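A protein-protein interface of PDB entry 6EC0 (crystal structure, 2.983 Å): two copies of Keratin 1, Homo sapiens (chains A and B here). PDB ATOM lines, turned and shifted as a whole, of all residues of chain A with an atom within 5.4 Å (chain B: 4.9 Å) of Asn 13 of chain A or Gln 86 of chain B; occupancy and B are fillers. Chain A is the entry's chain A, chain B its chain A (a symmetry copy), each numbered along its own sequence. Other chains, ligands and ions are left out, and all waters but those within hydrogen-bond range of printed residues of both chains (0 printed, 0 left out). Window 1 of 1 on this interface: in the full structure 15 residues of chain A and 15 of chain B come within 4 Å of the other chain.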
ATOM      1  N   GLU A   8     -29.074   2.297  11.581  1.00  0.00           N
ATOM      2  CA  GLU A   8     -30.066   3.350  11.396  1.00  0.00           C
ATOM      3  C   GLU A   8     -29.569   4.673  11.961  1.00  0.00           C
ATOM      4  O   GLU A   8     -29.688   5.719  11.315  1.00  0.00           O
ATOM      5  CB  GLU A   8     -31.384   2.941  12.056  1.00  0.00           C
ATOM      6  CG  GLU A   8     -32.024   1.679  11.465  1.00  0.00           C
ATOM      7  CD  GLU A   8     -33.328   1.287  12.147  1.00  0.00           C
ATOM      8  OE1 GLU A   8     -34.023   0.389  11.626  1.00  0.00           O
ATOM      9  OE2 GLU A   8     -33.659   1.874  13.198  1.00  0.00           O
ATOM     10  N   SER A   9     -29.008   4.646  13.172  1.00  0.00           N
ATOM     11  CA  SER A   9     -28.445   5.860  13.758  1.00  0.00           C
ATOM     12  C   SER A   9     -27.445   6.506  12.806  1.00  0.00           C
ATOM     13  O   SER A   9     -27.560   7.694  12.464  1.00  0.00           O
ATOM     14  CB  SER A   9     -27.793   5.518  15.100  1.00  0.00           C
ATOM     15  OG  SER A   9     -26.824   6.475  15.492  1.00  0.00           O
ATOM     16  N   PHE A  10     -26.478   5.720  12.332  1.00  0.00           N
ATOM     17  CA  PHE A  10     -25.437   6.279  11.481  1.00  0.00           C
ATOM     18  C   PHE A  10     -26.011   6.798  10.169  1.00  0.00           C
ATOM     19  O   PHE A  10     -25.605   7.862   9.688  1.00  0.00           O
ATOM     20  CB  PHE A  10     -24.367   5.226  11.223  1.00  0.00           C
ATOM     21  CG  PHE A  10     -23.128   5.773  10.602  1.00  0.00           C
ATOM     22  CD1 PHE A  10     -22.360   6.700  11.284  1.00  0.00           C
ATOM     23  CD2 PHE A  10     -22.726   5.363   9.342  1.00  0.00           C
ATOM     24  CE1 PHE A  10     -21.212   7.209  10.725  1.00  0.00           C
ATOM     25  CE2 PHE A  10     -21.578   5.869   8.777  1.00  0.00           C
ATOM     26  CZ  PHE A  10     -20.819   6.794   9.468  1.00  0.00           C
ATOM     27  N   ILE A  11     -26.949   6.059   9.572  1.00  0.00           N
ATOM     28  CA  ILE A  11     -27.588   6.530   8.346  1.00  0.00           C
ATOM     29  C   ILE A  11     -28.280   7.859   8.592  1.00  0.00           C
ATOM     30  O   ILE A  11     -28.261   8.741   7.734  1.00  0.00           O
ATOM     31  CB  ILE A  11     -28.575   5.481   7.794  1.00  0.00           C
ATOM     32  CG1 ILE A  11     -27.806   4.297   7.191  1.00  0.00           C
ATOM     33  CG2 ILE A  11     -29.519   6.134   6.770  1.00  0.00           C
ATOM     34  CD1 ILE A  11     -28.508   3.577   6.031  1.00  0.00           C
ATOM     35  N   ASN A  12     -28.933   8.016   9.745  1.00  0.00           N
ATOM     36  CA  ASN A  12     -29.611   9.277  10.033  1.00  0.00           C
ATOM     37  C   ASN A  12     -28.610  10.420  10.108  1.00  0.00           C
ATOM     38  O   ASN A  12     -28.820  11.485   9.513  1.00  0.00           O
ATOM     39  CB  ASN A  12     -30.418   9.164  11.328  1.00  0.00           C
ATOM     40  CG  ASN A  12     -31.882   8.838  11.073  1.00  0.00           C
ATOM     41  OD1 ASN A  12     -32.287   8.601   9.933  1.00  0.00           O
ATOM     42  ND2 ASN A  12     -32.683   8.817  12.134  1.00  0.00           N
ATOM     43  N   ASN A  13     -27.504  10.220  10.832  1.00  0.00           N
ATOM     44  CA  ASN A  13     -26.444  11.225  10.811  1.00  0.00           C
ATOM     45  C   ASN A  13     -26.022  11.552   9.374  1.00  0.00           C
ATOM     46  O   ASN A  13     -25.836  12.726   9.002  1.00  0.00           O
ATOM     47  CB  ASN A  13     -25.252  10.735  11.625  1.00  0.00           C
ATOM     48  CG  ASN A  13     -24.125  11.729  11.636  1.00  0.00           C
ATOM     49  OD1 ASN A  13     -24.277  12.858  11.167  1.00  0.00           O
ATOM     50  ND2 ASN A  13     -22.985  11.324  12.170  1.00  0.00           N
ATOM     51  N   LEU A  14     -25.878  10.520   8.544  1.00  0.00           N
ATOM     52  CA  LEU A  14     -25.503  10.739   7.156  1.00  0.00           C
ATOM     53  C   LEU A  14     -26.546  11.609   6.445  1.00  0.00           C
ATOM     54  O   LEU A  14     -26.219  12.670   5.892  1.00  0.00           O
ATOM     55  CB  LEU A  14     -25.309   9.379   6.480  1.00  0.00           C
ATOM     56  CG  LEU A  14     -24.875   9.318   5.033  1.00  0.00           C
ATOM     57  CD1 LEU A  14     -24.516   7.898   4.638  1.00  0.00           C
ATOM     58  CD2 LEU A  14     -26.021   9.833   4.181  1.00  0.00           C
ATOM     59  N   ARG A  15     -27.816  11.182   6.468  1.00  0.00           N
ATOM     60  CA  ARG A  15     -28.887  11.947   5.832  1.00  0.00           C
ATOM     61  C   ARG A  15     -28.875  13.395   6.295  1.00  0.00           C
ATOM     62  O   ARG A  15     -29.255  14.296   5.535  1.00  0.00           O
ATOM     63  CB  ARG A  15     -30.256  11.312   6.107  1.00  0.00           C
ATOM     64  CG  ARG A  15     -30.540  10.061   5.268  1.00  0.00           C
ATOM     65  CD  ARG A  15     -32.023   9.678   5.255  1.00  0.00           C
ATOM     66  NE  ARG A  15     -32.285   8.503   4.422  1.00  0.00           N
ATOM     67  CZ  ARG A  15     -33.376   7.743   4.507  1.00  0.00           C
ATOM     68  NH1 ARG A  15     -33.525   6.698   3.703  1.00  0.00           N
ATOM     69  NH2 ARG A  15     -34.317   8.017   5.402  1.00  0.00           N
ATOM     70  N   ARG A  16     -28.428  13.635   7.531  1.00  0.00           N
ATOM     71  CA  ARG A  16     -28.197  15.001   7.995  1.00  0.00           C
ATOM     72  C   ARG A  16     -27.152  15.699   7.126  1.00  0.00           C
ATOM     73  O   ARG A  16     -27.410  16.779   6.565  1.00  0.00           O
ATOM     74  CB  ARG A  16     -27.782  14.980   9.471  1.00  0.00           C
ATOM     75  CG  ARG A  16     -27.230  16.293  10.014  1.00  0.00           C
ATOM     76  CD  ARG A  16     -26.790  16.170  11.468  1.00  0.00           C
ATOM     77  NE  ARG A  16     -27.773  15.484  12.301  1.00  0.00           N
ATOM     78  CZ  ARG A  16     -27.587  15.183  13.583  1.00  0.00           C
ATOM     79  NH1 ARG A  16     -26.451  15.504  14.189  1.00  0.00           N
ATOM     80  NH2 ARG A  16     -28.538  14.556  14.260  1.00  0.00           N
ATOM     81  N   ARG A  17     -25.966  15.087   6.976  1.00  0.00           N
ATOM     82  CA  ARG A  17     -24.937  15.739   6.157  1.00  0.00           C
ATOM     83  C   ARG A  17     -25.445  16.035   4.746  1.00  0.00           C
ATOM     84  O   ARG A  17     -25.216  17.133   4.219  1.00  0.00           O
ATOM     85  CB  ARG A  17     -23.661  14.895   6.086  1.00  0.00           C
ATOM     86  CG  ARG A  17     -22.882  14.818   7.396  1.00  0.00           C
ATOM     87  CD  ARG A  17     -21.522  14.162   7.209  1.00  0.00           C
ATOM     88  NE  ARG A  17     -20.555  15.036   6.551  1.00  0.00           N
ATOM     89  CZ  ARG A  17     -19.388  14.621   6.062  1.00  0.00           C
ATOM     90  NH1 ARG A  17     -19.044  13.340   6.147  1.00  0.00           N
ATOM     91  NH2 ARG A  17     -18.563  15.484   5.483  1.00  0.00           N
ATOM     92  N   LEU B  81     -11.738  12.036   3.963  1.00  0.00           N
ATOM     93  CA  LEU B  81     -11.372  11.869   5.368  1.00  0.00           C
ATOM     94  C   LEU B  81     -12.612  11.840   6.238  1.00  0.00           C
ATOM     95  O   LEU B  81     -12.795  10.929   7.052  1.00  0.00           O
ATOM     96  CB  LEU B  81     -10.447  13.001   5.830  1.00  0.00           C
ATOM     97  CG  LEU B  81     -10.439  13.268   7.347  1.00  0.00           C
ATOM     98  CD1 LEU B  81      -9.983  12.037   8.065  1.00  0.00           C
ATOM     99  CD2 LEU B  81      -9.553  14.435   7.749  1.00  0.00           C
ATOM    100  N   ASP B  82     -13.463  12.857   6.103  1.00  0.00           N
ATOM    101  CA  ASP B  82     -14.714  12.874   6.850  1.00  0.00           C
ATOM    102  C   ASP B  82     -15.410  11.521   6.742  1.00  0.00           C
ATOM    103  O   ASP B  82     -15.894  10.972   7.744  1.00  0.00           O
ATOM    104  CB  ASP B  82     -15.616  13.996   6.326  1.00  0.00           C
ATOM    105  CG  ASP B  82     -14.985  15.385   6.442  1.00  0.00           C
ATOM    106  OD1 ASP B  82     -13.754  15.481   6.626  1.00  0.00           O
ATOM    107  OD2 ASP B  82     -15.729  16.387   6.334  1.00  0.00           O
ATOM    108  N   ASN B  83     -15.423  10.944   5.535  1.00  0.00           N
ATOM    109  CA  ASN B  83     -16.030   9.630   5.337  1.00  0.00           C
ATOM    110  C   ASN B  83     -15.319   8.566   6.162  1.00  0.00           C
ATOM    111  O   ASN B  83     -15.960   7.820   6.913  1.00  0.00           O
ATOM    112  CB  ASN B  83     -16.013   9.250   3.852  1.00  0.00           C
ATOM    113  CG  ASN B  83     -17.096   9.961   3.049  1.00  0.00           C
ATOM    114  OD1 ASN B  83     -17.678  10.943   3.505  1.00  0.00           O
ATOM    115  ND2 ASN B  83     -17.367   9.463   1.845  1.00  0.00           N
ATOM    116  N   LEU B  84     -13.994   8.478   6.041  1.00  0.00           N
ATOM    117  CA  LEU B  84     -13.280   7.413   6.733  1.00  0.00           C
ATOM    118  C   LEU B  84     -13.482   7.519   8.240  1.00  0.00           C
ATOM    119  O   LEU B  84     -13.814   6.529   8.893  1.00  0.00           O
ATOM    120  CB  LEU B  84     -11.788   7.427   6.375  1.00  0.00           C
ATOM    121  CG  LEU B  84     -11.429   6.995   4.943  1.00  0.00           C
ATOM    122  CD1 LEU B  84      -9.929   6.723   4.820  1.00  0.00           C
ATOM    123  CD2 LEU B  84     -12.222   5.764   4.466  1.00  0.00           C
ATOM    124  N   GLN B  85     -13.316   8.716   8.806  1.00  0.00           N
ATOM    125  CA  GLN B  85     -13.452   8.877  10.253  1.00  0.00           C
ATOM    126  C   GLN B  85     -14.860   8.518  10.715  1.00  0.00           C
ATOM    127  O   GLN B  85     -15.041   7.711  11.642  1.00  0.00           O
ATOM    128  CB  GLN B  85     -13.093  10.307  10.664  1.00  0.00           C
ATOM    129  CG  GLN B  85     -13.326  10.632  12.155  1.00  0.00           C
ATOM    130  CD  GLN B  85     -12.452   9.800  13.090  1.00  0.00           C
ATOM    131  OE1 GLN B  85     -11.560   9.077  12.643  1.00  0.00           O
ATOM    132  NE2 GLN B  85     -12.703   9.900  14.392  1.00  0.00           N
ATOM    133  N   GLN B  86     -15.879   9.116  10.086  1.00  0.00           N
ATOM    134  CA  GLN B  86     -17.248   8.790  10.465  1.00  0.00           C
ATOM    135  C   GLN B  86     -17.451   7.277  10.445  1.00  0.00           C
ATOM    136  O   GLN B  86     -17.974   6.687  11.406  1.00  0.00           O
ATOM    137  CB  GLN B  86     -18.233   9.498   9.525  1.00  0.00           C
ATOM    138  CG  GLN B  86     -18.214  11.034   9.604  1.00  0.00           C
ATOM    139  CD  GLN B  86     -18.866  11.567  10.870  1.00  0.00           C
ATOM    140  OE1 GLN B  86     -19.259  10.803  11.750  1.00  0.00           O
ATOM    141  NE2 GLN B  86     -18.991  12.884  10.962  1.00  0.00           N
ATOM    142  N   GLU B  87     -16.981   6.627   9.375  1.00  0.00           N
ATOM    143  CA  GLU B  87     -17.097   5.176   9.272  1.00  0.00           C
ATOM    144  C   GLU B  87     -16.370   4.483  10.415  1.00  0.00           C
ATOM    145  O   GLU B  87     -16.827   3.447  10.909  1.00  0.00           O
ATOM    146  CB  GLU B  87     -16.548   4.696   7.928  1.00  0.00           C
ATOM    147  CG  GLU B  87     -16.743   3.204   7.688  1.00  0.00           C
ATOM    148  CD  GLU B  87     -16.300   2.762   6.307  1.00  0.00           C
ATOM    149  OE1 GLU B  87     -15.234   3.221   5.847  1.00  0.00           O
ATOM    150  OE2 GLU B  87     -17.021   1.957   5.680  1.00  0.00           O
ATOM    151  N   ILE B  88     -15.231   5.031  10.844  1.00  0.00           N
ATOM    152  CA  ILE B  88     -14.511   4.453  11.974  1.00  0.00           C
ATOM    153  C   ILE B  88     -15.418   4.446  13.195  1.00  0.00           C
ATOM    154  O   ILE B  88     -15.844   3.386  13.663  1.00  0.00           O
ATOM    155  CB  ILE B  88     -13.200   5.215  12.250  1.00  0.00           C
ATOM    156  CG1 ILE B  88     -12.224   5.118  11.070  1.00  0.00           C
ATOM    157  CG2 ILE B  88     -12.501   4.678  13.507  1.00  0.00           C
ATOM    158  CD1 ILE B  88     -12.184   3.775  10.363  1.00  0.00           C
ATOM    159  N   ASP B  89     -15.764   5.639  13.693  1.00  0.00           N
ATOM    160  CA  ASP B  89     -16.615   5.734  14.877  1.00  0.00           C
ATOM    161  C   ASP B  89     -17.760   4.727  14.807  1.00  0.00           C
ATOM    162  O   ASP B  89     -17.956   3.896  15.718  1.00  0.00           O
ATOM    163  CB  ASP B  89     -17.163   7.159  15.000  1.00  0.00           C
ATOM    164  CG  ASP B  89     -16.070   8.212  15.068  1.00  0.00           C
ATOM    165  OD1 ASP B  89     -14.929   7.923  14.652  1.00  0.00           O
ATOM    166  OD2 ASP B  89     -16.358   9.337  15.527  1.00  0.00           O
ATOM    167  N   PHE B  90     -18.512   4.771  13.701  1.00  0.00           N
ATOM    168  CA  PHE B  90     -19.617   3.834  13.528  1.00  0.00           C
ATOM    169  C   PHE B  90     -19.157   2.398  13.749  1.00  0.00           C
ATOM    170  O   PHE B  90     -19.728   1.669  14.569  1.00  0.00           O
ATOM    171  CB  PHE B  90     -20.229   3.988  12.137  1.00  0.00           C
ATOM    172  CG  PHE B  90     -21.070   2.819  11.726  1.00  0.00           C
ATOM    173  CD1 PHE B  90     -22.341   2.646  12.255  1.00  0.00           C
ATOM    174  CD2 PHE B  90     -20.590   1.887  10.825  1.00  0.00           C
ATOM    175  CE1 PHE B  90     -23.117   1.565  11.884  1.00  0.00           C
ATOM    176  CE2 PHE B  90     -21.360   0.807  10.450  1.00  0.00           C
ATOM    177  CZ  PHE B  90     -22.626   0.644  10.979  1.00  0.00           C
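The side-chain carboxylate of Asp 82 of chain B lies within salt-bridge range of the guanidinium group of Arg 17 of chain A, 3.1 Å away.
Phe 10 of chain A touches Gln 86 of chain B (CE1 to O, 3.3 Å).
Glu 87 of chain B touches Phe 10 of chain A (N to CZ, 3.8 Å).
CD1 of Phe 90 of chain B touches CB of Phe 10 of chain A, 3.4 Å away.
Asn 13 of chain A touches Gln 86 of chain B (ND2 to OE1, 3.8 Å).
Asn 83 of chain B touches Arg 17 of chain A.
Of the printed residues of chain B, Phe 10 of chain A touches Gln 86, Glu 87 and Phe 90.
Of chain A, only Phe 10 (3.3 Å) and Asn 13 (3.8 Å) come within 4 Å of Gln 86 of chain B.
Printed residues of chain A within 4 Å of Phe 90 of chain B: Phe 10 (3.4 Å).
The nearest printed residue of chain B that does not touch Asn 13 of chain A is Asp 89 of chain B (7.7 Å).
The nearest residue of chain A that does not touch Gln 86 of chain B is Arg 17 of chain A (4.2 Å).
The nearest printed residue of chain B that does not touch Phe 10 of chain A is Asn 83 of chain B (5.6 Å).
Hydrophobic or aromatic side chains of chain B that line the printed part of chain A: Phe 90.
No position is printed for both chains.
Of the 6 pairs that touch across the chains among the printed residues, none has its exchanged pair printed and touching as well.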
